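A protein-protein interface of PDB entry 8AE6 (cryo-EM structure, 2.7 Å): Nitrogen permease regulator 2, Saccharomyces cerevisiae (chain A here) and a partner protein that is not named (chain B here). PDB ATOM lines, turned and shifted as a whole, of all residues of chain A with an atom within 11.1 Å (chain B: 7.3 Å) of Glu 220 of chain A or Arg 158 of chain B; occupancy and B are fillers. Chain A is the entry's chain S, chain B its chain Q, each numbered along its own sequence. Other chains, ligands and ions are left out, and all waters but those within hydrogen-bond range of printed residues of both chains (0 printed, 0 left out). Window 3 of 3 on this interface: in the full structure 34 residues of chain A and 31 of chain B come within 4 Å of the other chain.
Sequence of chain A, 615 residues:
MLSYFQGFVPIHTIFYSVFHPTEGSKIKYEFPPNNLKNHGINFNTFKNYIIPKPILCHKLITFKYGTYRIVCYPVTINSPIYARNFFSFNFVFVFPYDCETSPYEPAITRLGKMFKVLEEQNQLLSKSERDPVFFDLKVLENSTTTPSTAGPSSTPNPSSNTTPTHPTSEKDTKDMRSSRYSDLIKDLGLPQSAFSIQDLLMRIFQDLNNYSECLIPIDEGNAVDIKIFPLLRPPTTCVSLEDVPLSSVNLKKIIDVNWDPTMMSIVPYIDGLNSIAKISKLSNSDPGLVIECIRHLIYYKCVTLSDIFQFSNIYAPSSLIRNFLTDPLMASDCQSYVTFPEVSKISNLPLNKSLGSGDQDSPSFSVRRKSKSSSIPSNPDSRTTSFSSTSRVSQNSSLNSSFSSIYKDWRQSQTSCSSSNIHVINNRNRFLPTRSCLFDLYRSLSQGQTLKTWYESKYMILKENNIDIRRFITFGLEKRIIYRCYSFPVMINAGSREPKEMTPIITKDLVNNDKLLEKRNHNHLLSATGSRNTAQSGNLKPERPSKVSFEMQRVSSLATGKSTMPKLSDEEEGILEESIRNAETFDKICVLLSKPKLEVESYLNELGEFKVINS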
ATOM      1  N   LEU A 118      10.596  12.493 -20.997  1.00  0.00           N
ATOM      2  CA  LEU A 118      11.975  12.562 -20.514  1.00  0.00           C
ATOM      3  C   LEU A 118      12.149  11.851 -19.177  1.00  0.00           C
ATOM      4  O   LEU A 118      13.162  11.175 -18.956  1.00  0.00           O
ATOM      5  CB  LEU A 118      12.414  14.020 -20.409  1.00  0.00           C
ATOM      6  CG  LEU A 118      12.642  14.730 -21.740  1.00  0.00           C
ATOM      7  CD1 LEU A 118      13.237  16.094 -21.501  1.00  0.00           C
ATOM      8  CD2 LEU A 118      13.538  13.904 -22.640  1.00  0.00           C
ATOM      9  N   GLN A 121      12.095   8.206 -19.815  1.00  0.00           N
ATOM     10  CA  GLN A 121      13.256   7.741 -20.567  1.00  0.00           C
ATOM     11  C   GLN A 121      14.525   7.720 -19.721  1.00  0.00           C
ATOM     12  O   GLN A 121      15.122   6.658 -19.520  1.00  0.00           O
ATOM     13  CB  GLN A 121      13.454   8.623 -21.804  1.00  0.00           C
ATOM     14  CG  GLN A 121      14.552   8.153 -22.732  1.00  0.00           C
ATOM     15  CD  GLN A 121      15.171   9.287 -23.513  1.00  0.00           C
ATOM     16  OE1 GLN A 121      14.612  10.379 -23.594  1.00  0.00           O
ATOM     17  NE2 GLN A 121      16.334   9.037 -24.099  1.00  0.00           N
ATOM     18  N   ASN A 122      14.949   8.877 -19.212  1.00  0.00           N
ATOM     19  CA  ASN A 122      16.243   8.980 -18.547  1.00  0.00           C
ATOM     20  C   ASN A 122      16.148   9.451 -17.103  1.00  0.00           C
ATOM     21  O   ASN A 122      17.193   9.693 -16.483  1.00  0.00           O
ATOM     22  CB  ASN A 122      17.177   9.902 -19.337  1.00  0.00           C
ATOM     23  CG  ASN A 122      16.771  11.360 -19.257  1.00  0.00           C
ATOM     24  OD1 ASN A 122      17.215  12.091 -18.370  1.00  0.00           O
ATOM     25  ND2 ASN A 122      15.938  11.793 -20.191  1.00  0.00           N
ATOM     26  N   LEU A 124      14.889  12.348 -15.617  1.00  0.00           N
ATOM     27  CA  LEU A 124      15.499  13.669 -15.556  1.00  0.00           C
ATOM     28  C   LEU A 124      15.092  14.423 -14.292  1.00  0.00           C
ATOM     29  O   LEU A 124      15.947  14.810 -13.484  1.00  0.00           O
ATOM     30  CB  LEU A 124      15.123  14.436 -16.831  1.00  0.00           C
ATOM     31  CG  LEU A 124      15.661  15.809 -17.208  1.00  0.00           C
ATOM     32  CD1 LEU A 124      15.709  15.917 -18.705  1.00  0.00           C
ATOM     33  CD2 LEU A 124      14.707  16.853 -16.696  1.00  0.00           C
ATOM     34  N   LYS A 127      16.043  12.660 -10.867  1.00  0.00           N
ATOM     35  CA  LYS A 127      17.455  12.766 -10.533  1.00  0.00           C
ATOM     36  C   LYS A 127      17.898  14.203 -10.304  1.00  0.00           C
ATOM     37  O   LYS A 127      18.935  14.418  -9.666  1.00  0.00           O
ATOM     38  CB  LYS A 127      18.314  12.142 -11.631  1.00  0.00           C
ATOM     39  CG  LYS A 127      18.299  10.630 -11.653  1.00  0.00           C
ATOM     40  CD  LYS A 127      19.511  10.073 -12.379  1.00  0.00           C
ATOM     41  CE  LYS A 127      19.717  10.737 -13.731  1.00  0.00           C
ATOM     42  NZ  LYS A 127      18.599  10.445 -14.664  1.00  0.00           N
ATOM     43  N   ARG A 130      18.606  15.573  -6.530  1.00  0.00           N
ATOM     44  CA  ARG A 130      19.846  15.222  -5.825  1.00  0.00           C
ATOM     45  C   ARG A 130      19.574  14.728  -4.405  1.00  0.00           C
ATOM     46  O   ARG A 130      20.305  15.043  -3.465  1.00  0.00           O
ATOM     47  CB  ARG A 130      20.841  16.385  -5.819  1.00  0.00           C
ATOM     48  CG  ARG A 130      21.401  16.720  -7.189  1.00  0.00           C
ATOM     49  CD  ARG A 130      22.066  15.508  -7.822  1.00  0.00           C
ATOM     50  NE  ARG A 130      22.887  15.871  -8.970  1.00  0.00           N
ATOM     51  CZ  ARG A 130      22.580  15.593 -10.229  1.00  0.00           C
ATOM     52  NH1 ARG A 130      21.468  14.948 -10.542  1.00  0.00           N
ATOM     53  NH2 ARG A 130      23.405  15.974 -11.200  1.00  0.00           N
ATOM     54  N   PHE A 195      21.853  20.298 -15.345  1.00  0.00           N
ATOM     55  CA  PHE A 195      20.552  20.880 -15.653  1.00  0.00           C
ATOM     56  C   PHE A 195      19.928  21.491 -14.403  1.00  0.00           C
ATOM     57  O   PHE A 195      19.941  20.885 -13.333  1.00  0.00           O
ATOM     58  CB  PHE A 195      19.621  19.822 -16.250  1.00  0.00           C
ATOM     59  CG  PHE A 195      18.201  20.276 -16.374  1.00  0.00           C
ATOM     60  CD1 PHE A 195      17.881  21.394 -17.130  1.00  0.00           C
ATOM     61  CD2 PHE A 195      17.187  19.604 -15.722  1.00  0.00           C
ATOM     62  CE1 PHE A 195      16.574  21.821 -17.233  1.00  0.00           C
ATOM     63  CE2 PHE A 195      15.882  20.032 -15.822  1.00  0.00           C
ATOM     64  CZ  PHE A 195      15.576  21.134 -16.581  1.00  0.00           C
ATOM     65  N   ARG A 203      14.024  31.128 -17.786  1.00  0.00           N
ATOM     66  CA  ARG A 203      14.097  31.280 -19.231  1.00  0.00           C
ATOM     67  C   ARG A 203      12.726  31.137 -19.878  1.00  0.00           C
ATOM     68  O   ARG A 203      12.380  31.924 -20.766  1.00  0.00           O
ATOM     69  CB  ARG A 203      15.083  30.265 -19.804  1.00  0.00           C
ATOM     70  CG  ARG A 203      16.538  30.655 -19.656  1.00  0.00           C
ATOM     71  CD  ARG A 203      16.936  31.708 -20.675  1.00  0.00           C
ATOM     72  NE  ARG A 203      16.968  31.183 -22.035  1.00  0.00           N
ATOM     73  CZ  ARG A 203      17.973  30.488 -22.551  1.00  0.00           C
ATOM     74  NH1 ARG A 203      19.054  30.206 -21.842  1.00  0.00           N
ATOM     75  NH2 ARG A 203      17.893  30.068 -23.808  1.00  0.00           N
ATOM     76  N   ASP A 207      11.167  34.381 -21.684  1.00  0.00           N
ATOM     77  CA  ASP A 207      11.066  34.224 -23.126  1.00  0.00           C
ATOM     78  C   ASP A 207       9.613  34.218 -23.585  1.00  0.00           C
ATOM     79  O   ASP A 207       9.296  34.761 -24.649  1.00  0.00           O
ATOM     80  CB  ASP A 207      11.786  32.951 -23.561  1.00  0.00           C
ATOM     81  CG  ASP A 207      13.293  33.086 -23.499  1.00  0.00           C
ATOM     82  OD1 ASP A 207      13.782  34.206 -23.245  1.00  0.00           O
ATOM     83  OD2 ASP A 207      13.990  32.070 -23.705  1.00  0.00           O
ATOM     84  N   CYS A 214      10.299  30.536 -27.315  1.00  0.00           N
ATOM     85  CA  CYS A 214      11.455  30.138 -26.526  1.00  0.00           C
ATOM     86  C   CYS A 214      12.183  28.997 -27.219  1.00  0.00           C
ATOM     87  O   CYS A 214      11.574  28.195 -27.930  1.00  0.00           O
ATOM     88  CB  CYS A 214      11.055  29.733 -25.101  1.00  0.00           C
ATOM     89  SG  CYS A 214      10.416  28.066 -24.902  1.00  0.00           S
ATOM     90  N   LEU A 215      13.500  28.954 -27.016  1.00  0.00           N
ATOM     91  CA  LEU A 215      14.346  27.831 -27.428  1.00  0.00           C
ATOM     92  C   LEU A 215      15.387  27.676 -26.323  1.00  0.00           C
ATOM     93  O   LEU A 215      16.429  28.335 -26.337  1.00  0.00           O
ATOM     94  CB  LEU A 215      14.985  28.058 -28.790  1.00  0.00           C
ATOM     95  CG  LEU A 215      15.572  26.840 -29.506  1.00  0.00           C
ATOM     96  CD1 LEU A 215      15.319  26.945 -30.993  1.00  0.00           C
ATOM     97  CD2 LEU A 215      17.059  26.705 -29.241  1.00  0.00           C
ATOM     98  N   ILE A 216      15.091  26.808 -25.361  1.00  0.00           N
ATOM     99  CA  ILE A 216      15.888  26.675 -24.148  1.00  0.00           C
ATOM    100  C   ILE A 216      16.467  25.271 -24.081  1.00  0.00           C
ATOM    101  O   ILE A 216      15.741  24.320 -23.760  1.00  0.00           O
ATOM    102  CB  ILE A 216      15.041  26.978 -22.907  1.00  0.00           C
ATOM    103  CG1 ILE A 216      14.387  28.347 -23.055  1.00  0.00           C
ATOM    104  CG2 ILE A 216      15.895  26.933 -21.662  1.00  0.00           C
ATOM    105  CD1 ILE A 216      13.129  28.488 -22.278  1.00  0.00           C
ATOM    106  N   PRO A 217      17.752  25.084 -24.380  1.00  0.00           N
ATOM    107  CA  PRO A 217      18.331  23.737 -24.334  1.00  0.00           C
ATOM    108  C   PRO A 217      18.504  23.265 -22.899  1.00  0.00           C
ATOM    109  O   PRO A 217      19.066  23.972 -22.059  1.00  0.00           O
ATOM    110  CB  PRO A 217      19.684  23.903 -25.038  1.00  0.00           C
ATOM    111  CG  PRO A 217      19.639  25.248 -25.680  1.00  0.00           C
ATOM    112  CD  PRO A 217      18.718  26.077 -24.867  1.00  0.00           C
ATOM    113  N   ILE A 218      18.013  22.062 -22.626  1.00  0.00           N
ATOM    114  CA  ILE A 218      18.132  21.468 -21.302  1.00  0.00           C
ATOM    115  C   ILE A 218      19.089  20.287 -21.278  1.00  0.00           C
ATOM    116  O   ILE A 218      19.489  19.861 -20.183  1.00  0.00           O
ATOM    117  CB  ILE A 218      16.753  21.049 -20.753  1.00  0.00           C
ATOM    118  CG1 ILE A 218      16.180  19.892 -21.568  1.00  0.00           C
ATOM    119  CG2 ILE A 218      15.799  22.226 -20.774  1.00  0.00           C
ATOM    120  CD1 ILE A 218      14.809  19.459 -21.122  1.00  0.00           C
ATOM    121  N   ASP A 219      19.478  19.753 -22.430  1.00  0.00           N
ATOM    122  CA  ASP A 219      20.394  18.628 -22.511  1.00  0.00           C
ATOM    123  C   ASP A 219      21.191  18.757 -23.802  1.00  0.00           C
ATOM    124  O   ASP A 219      21.198  19.810 -24.443  1.00  0.00           O
ATOM    125  CB  ASP A 219      19.637  17.294 -22.448  1.00  0.00           C
ATOM    126  CG  ASP A 219      19.402  16.819 -21.032  1.00  0.00           C
ATOM    127  OD1 ASP A 219      20.283  17.042 -20.174  1.00  0.00           O
ATOM    128  OD2 ASP A 219      18.342  16.212 -20.778  1.00  0.00           O
ATOM    129  N   GLU A 220      21.866  17.676 -24.181  1.00  0.00           N
ATOM    130  CA  GLU A 220      22.582  17.632 -25.448  1.00  0.00           C
ATOM    131  C   GLU A 220      21.681  17.274 -26.619  1.00  0.00           C
ATOM    132  O   GLU A 220      22.125  17.363 -27.767  1.00  0.00           O
ATOM    133  CB  GLU A 220      23.736  16.632 -25.363  1.00  0.00           C
ATOM    134  CG  GLU A 220      24.728  16.921 -24.251  1.00  0.00           C
ATOM    135  CD  GLU A 220      24.478  16.085 -23.012  1.00  0.00           C
ATOM    136  OE1 GLU A 220      23.742  15.080 -23.111  1.00  0.00           O
ATOM    137  OE2 GLU A 220      25.014  16.433 -21.940  1.00  0.00           O
ATOM    138  N   GLY A 221      20.441  16.869 -26.361  1.00  0.00           N
ATOM    139  CA  GLY A 221      19.518  16.544 -27.427  1.00  0.00           C
ATOM    140  C   GLY A 221      18.104  17.030 -27.180  1.00  0.00           C
ATOM    141  O   GLY A 221      17.222  16.838 -28.020  1.00  0.00           O
ATOM    142  N   ASN A 222      17.878  17.673 -26.040  1.00  0.00           N
ATOM    143  CA  ASN A 222      16.549  18.112 -25.643  1.00  0.00           C
ATOM    144  C   ASN A 222      16.530  19.619 -25.453  1.00  0.00           C
ATOM    145  O   ASN A 222      17.469  20.200 -24.901  1.00  0.00           O
ATOM    146  CB  ASN A 222      16.107  17.423 -24.356  1.00  0.00           C
ATOM    147  CG  ASN A 222      15.762  15.971 -24.564  1.00  0.00           C
ATOM    148  OD1 ASN A 222      14.812  15.644 -25.272  1.00  0.00           O
ATOM    149  ND2 ASN A 222      16.534  15.086 -23.947  1.00  0.00           N
ATOM    150  N   ALA A 223      15.453  20.247 -25.913  1.00  0.00           N
ATOM    151  CA  ALA A 223      15.265  21.677 -25.753  1.00  0.00           C
ATOM    152  C   ALA A 223      13.778  21.966 -25.647  1.00  0.00           C
ATOM    153  O   ALA A 223      12.947  21.209 -26.155  1.00  0.00           O
ATOM    154  CB  ALA A 223      15.874  22.462 -26.920  1.00  0.00           C
ATOM    155  N   VAL A 224      13.452  23.063 -24.981  1.00  0.00           N
ATOM    156  CA  VAL A 224      12.077  23.517 -24.831  1.00  0.00           C
ATOM    157  C   VAL A 224      11.822  24.513 -25.955  1.00  0.00           C
ATOM    158  O   VAL A 224      12.304  25.646 -25.916  1.00  0.00           O
ATOM    159  CB  VAL A 224      11.828  24.131 -23.453  1.00  0.00           C
ATOM    160  CG1 VAL A 224      10.401  24.627 -23.344  1.00  0.00           C
ATOM    161  CG2 VAL A 224      12.120  23.118 -22.367  1.00  0.00           C
ATOM    162  N   ASP A 225      11.076  24.086 -26.969  1.00  0.00           N
ATOM    163  CA  ASP A 225      10.720  24.928 -28.108  1.00  0.00           C
ATOM    164  C   ASP A 225       9.219  25.175 -28.054  1.00  0.00           C
ATOM    165  O   ASP A 225       8.423  24.319 -28.449  1.00  0.00           O
ATOM    166  CB  ASP A 225      11.127  24.275 -29.427  1.00  0.00           C
ATOM    167  CG  ASP A 225      12.596  23.912 -29.469  1.00  0.00           C
ATOM    168  OD1 ASP A 225      13.374  24.455 -28.656  1.00  0.00           O
ATOM    169  OD2 ASP A 225      12.979  23.082 -30.321  1.00  0.00           O
ATOM    170  N   VAL B 135      15.532  33.876 -31.927  1.00  0.00           N
ATOM    171  CA  VAL B 135      15.338  32.638 -31.183  1.00  0.00           C
ATOM    172  C   VAL B 135      15.746  31.417 -32.004  1.00  0.00           C
ATOM    173  O   VAL B 135      16.108  30.381 -31.432  1.00  0.00           O
ATOM    174  CB  VAL B 135      13.871  32.556 -30.707  1.00  0.00           C
ATOM    175  CG1 VAL B 135      13.654  31.426 -29.717  1.00  0.00           C
ATOM    176  CG2 VAL B 135      13.463  33.863 -30.062  1.00  0.00           C
ATOM    177  N   THR B 137      18.398  30.666 -33.358  1.00  0.00           N
ATOM    178  CA  THR B 137      19.854  30.507 -33.291  1.00  0.00           C
ATOM    179  C   THR B 137      20.525  30.984 -34.578  1.00  0.00           C
ATOM    180  O   THR B 137      21.153  30.215 -35.302  1.00  0.00           O
ATOM    181  CB  THR B 137      20.254  29.061 -32.966  1.00  0.00           C
ATOM    182  OG1 THR B 137      20.089  28.245 -34.133  1.00  0.00           O
ATOM    183  CG2 THR B 137      19.408  28.492 -31.832  1.00  0.00           C
ATOM    184  N   SER B 155      25.730  31.476 -36.682  1.00  0.00           N
ATOM    185  CA  SER B 155      24.835  30.771 -35.780  1.00  0.00           C
ATOM    186  C   SER B 155      25.627  30.164 -34.635  1.00  0.00           C
ATOM    187  O   SER B 155      26.830  29.920 -34.742  1.00  0.00           O
ATOM    188  CB  SER B 155      24.064  29.678 -36.521  1.00  0.00           C
ATOM    189  OG  SER B 155      23.275  28.915 -35.625  1.00  0.00           O
ATOM    190  N   SER B 156      24.926  29.918 -33.527  1.00  0.00           N
ATOM    191  CA  SER B 156      25.475  29.150 -32.418  1.00  0.00           C
ATOM    192  C   SER B 156      25.028  27.700 -32.428  1.00  0.00           C
ATOM    193  O   SER B 156      25.649  26.872 -31.750  1.00  0.00           O
ATOM    194  CB  SER B 156      25.080  29.783 -31.082  1.00  0.00           C
ATOM    195  OG  SER B 156      23.676  29.913 -30.981  1.00  0.00           O
ATOM    196  N   TRP B 157      23.943  27.393 -33.139  1.00  0.00           N
ATOM    197  CA  TRP B 157      23.400  26.071 -33.443  1.00  0.00           C
ATOM    198  C   TRP B 157      22.819  25.335 -32.241  1.00  0.00           C
ATOM    199  O   TRP B 157      22.239  24.260 -32.423  1.00  0.00           O
ATOM    200  CB  TRP B 157      24.433  25.156 -34.114  1.00  0.00           C
ATOM    201  CG  TRP B 157      25.161  25.798 -35.244  1.00  0.00           C
ATOM    202  CD1 TRP B 157      26.455  26.222 -35.246  1.00  0.00           C
ATOM    203  CD2 TRP B 157      24.644  26.080 -36.547  1.00  0.00           C
ATOM    204  NE1 TRP B 157      26.775  26.755 -36.468  1.00  0.00           N
ATOM    205  CE2 TRP B 157      25.680  26.678 -37.286  1.00  0.00           C
ATOM    206  CE3 TRP B 157      23.403  25.886 -37.160  1.00  0.00           C
ATOM    207  CZ2 TRP B 157      25.515  27.088 -38.605  1.00  0.00           C
ATOM    208  CZ3 TRP B 157      23.241  26.291 -38.471  1.00  0.00           C
ATOM    209  CH2 TRP B 157      24.291  26.885 -39.178  1.00  0.00           C
ATOM    210  N   ARG B 158      22.946  25.863 -31.025  1.00  0.00           N
ATOM    211  CA  ARG B 158      22.396  25.191 -29.857  1.00  0.00           C
ATOM    212  C   ARG B 158      21.351  26.016 -29.126  1.00  0.00           C
ATOM    213  O   ARG B 158      20.233  25.538 -28.909  1.00  0.00           O
ATOM    214  CB  ARG B 158      23.527  24.805 -28.889  1.00  0.00           C
ATOM    215  CG  ARG B 158      24.061  23.392 -29.095  1.00  0.00           C
ATOM    216  CD  ARG B 158      22.933  22.369 -29.099  1.00  0.00           C
ATOM    217  NE  ARG B 158      23.385  21.048 -29.519  1.00  0.00           N
ATOM    218  CZ  ARG B 158      23.811  20.103 -28.691  1.00  0.00           C
ATOM    219  NH1 ARG B 158      23.851  20.299 -27.384  1.00  0.00           N
ATOM    220  NH2 ARG B 158      24.202  18.934 -29.189  1.00  0.00           N
ATOM    221  N   SER B 159      21.673  27.249 -28.752  1.00  0.00           N
ATOM    222  CA  SER B 159      20.836  28.032 -27.857  1.00  0.00           C
ATOM    223  C   SER B 159      20.368  29.312 -28.532  1.00  0.00           C
ATOM    224  O   SER B 159      21.076  29.892 -29.361  1.00  0.00           O
ATOM    225  CB  SER B 159      21.584  28.379 -26.568  1.00  0.00           C
ATOM    226  OG  SER B 159      20.838  29.288 -25.778  1.00  0.00           O
ATOM    227  N   ALA B 160      19.166  29.740 -28.159  1.00  0.00           N
ATOM    228  CA  ALA B 160      18.582  30.954 -28.711  1.00  0.00           C
ATOM    229  C   ALA B 160      19.358  32.181 -28.256  1.00  0.00           C
ATOM    230  O   ALA B 160      19.799  32.269 -27.106  1.00  0.00           O
ATOM    231  CB  ALA B 160      17.122  31.077 -28.288  1.00  0.00           C
ATOM    232  N   HIS B 178      24.235  33.572 -26.339  1.00  0.00           N
ATOM    233  CA  HIS B 178      23.317  32.465 -26.592  1.00  0.00           C
ATOM    234  C   HIS B 178      23.261  31.611 -25.331  1.00  0.00           C
ATOM    235  O   HIS B 178      24.041  30.669 -25.174  1.00  0.00           O
ATOM    236  CB  HIS B 178      23.765  31.637 -27.788  1.00  0.00           C
ATOM    237  CG  HIS B 178      23.880  32.415 -29.061  1.00  0.00           C
ATOM    238  ND1 HIS B 178      23.006  32.251 -30.113  1.00  0.00           N
ATOM    239  CD2 HIS B 178      24.781  33.340 -29.463  1.00  0.00           C
ATOM    240  CE1 HIS B 178      23.358  33.049 -31.104  1.00  0.00           C
ATOM    241  NE2 HIS B 178      24.431  33.723 -30.735  1.00  0.00           N
ATOM    242  N   ASP B 181      26.547  31.215 -22.960  1.00  0.00           N
ATOM    243  CA  ASP B 181      27.773  31.440 -23.708  1.00  0.00           C
ATOM    244  C   ASP B 181      27.718  32.763 -24.455  1.00  0.00           C
ATOM    245  O   ASP B 181      26.650  33.214 -24.876  1.00  0.00           O
ATOM    246  CB  ASP B 181      28.021  30.302 -24.700  1.00  0.00           C
ATOM    247  CG  ASP B 181      28.034  28.942 -24.033  1.00  0.00           C
ATOM    248  OD1 ASP B 181      28.437  28.858 -22.855  1.00  0.00           O
ATOM    249  OD2 ASP B 181      27.641  27.955 -24.689  1.00  0.00           O
ATOM    250  N   PHE B 183      29.640  34.480 -27.758  1.00  0.00           N
ATOM    251  CA  PHE B 183      30.489  34.235 -28.916  1.00  0.00           C
ATOM    252  C   PHE B 183      30.809  35.560 -29.588  1.00  0.00           C
ATOM    253  O   PHE B 183      29.908  36.371 -29.823  1.00  0.00           O
ATOM    254  CB  PHE B 183      29.811  33.300 -29.915  1.00  0.00           C
ATOM    255  CG  PHE B 183      29.500  31.942 -29.370  1.00  0.00           C
ATOM    256  CD1 PHE B 183      30.491  30.988 -29.248  1.00  0.00           C
ATOM    257  CD2 PHE B 183      28.212  31.611 -29.001  1.00  0.00           C
ATOM    258  CE1 PHE B 183      30.205  29.733 -28.751  1.00  0.00           C
ATOM    259  CE2 PHE B 183      27.918  30.361 -28.506  1.00  0.00           C
ATOM    260  CZ  PHE B 183      28.916  29.421 -28.382  1.00  0.00           C
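The backbone carbonyl oxygen (O) of Glu 220 of chain A is in hydrogen-bond range of the guanidinium group (NH2) of Arg 158 of chain B, 3.0 Å away.
The backbone carbonyl oxygen of Thr 137 of chain B lies within hydrogen-bond range of the side-chain hydroxyl of Ser 155 of chain B, at 2.5 Å.
O of Val 224 of chain A sits at hydrogen-bond distance from SG of Cys 214 of chain A, 3.2 Å away.
ND1 of His 178 of chain B lies within hydrogen-bond range of O of Ser 159 of chain B (3.1 Å).
O of Ser 159 of chain B lies within hydrogen-bond range of OG of Ser 156 of chain B (3.1 Å).
NH2 of Arg 203 of chain A sits at hydrogen-bond distance from O of Leu 215 of chain A.
The side-chain carboxylate of Asp 207 of chain A is in salt-bridge range of the guanidinium group of Arg 203 of chain A.
Among the printed residues, merely in contact across the chains: Pro 217 of chain A with Arg 158 of chain B (3.3 Å), Leu 215 of chain A with Arg 158 of chain B (3.4 Å), Leu 215 of chain A with Ala 160 of chain B (3.4 Å), Leu 215 of chain A with Val 135 of chain B (3.6 Å), Arg 203 of chain A with Ser 159 of chain B (3.6 Å), Pro 217 of chain A with Ser 159 of chain B (3.7 Å), Cys 214 of chain A with Val 135 of chain B (3.8 Å), Leu 215 of chain A with Thr 137 of chain B (3.9 Å) and Asp 219 of chain A with Arg 158 of chain B (3.99 Å).
Of the printed residues of chain B, Leu 215 of chain A touches Val 135, Thr 137, Arg 158 and Ala 160.
Ile 216 of chain A touches none of the printed residues of chain B.
Of chain B, only Arg 158 comes within 4 Å of Glu 220 of chain A.
Of the printed residues of chain A, Val 135 of chain B touches Cys 214 and Leu 215.
Of the printed residues of chain A, Thr 137 of chain B touches Leu 215 (3.9 Å).
Of the printed residues of chain A, Arg 158 of chain B touches Leu 215, Pro 217, Asp 219 and Glu 220.
Of chain A, only Arg 203 (3.6 Å) and Pro 217 (3.7 Å) come within 4 Å of Ser 159 of chain B.
The nearest printed residue of chain B that does not touch Glu 220 of chain A is Trp 157 of chain B (8.3 Å).
The nearest printed residue of chain B that does not touch Arg 203 of chain A is Ala 160 of chain B (4.4 Å).
Printed residues of chain B that touch a printed residue of chain A: Val 135, Thr 137, Arg 158, Ser 159 and Ala 160.
Hydrophobic or aromatic side chains of chain B that line the printed part of chain A: Val 135 and Ala 160.
Of the 21 printed residues of chain A, 6 touch a printed residue of chain B.
Among the printed residues, 10 pairs touch across the chains.
Among the printed residues, no Asp or Glu carboxylate lies within 4 Å of a Lys or Arg side-chain nitrogen of the other chain.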
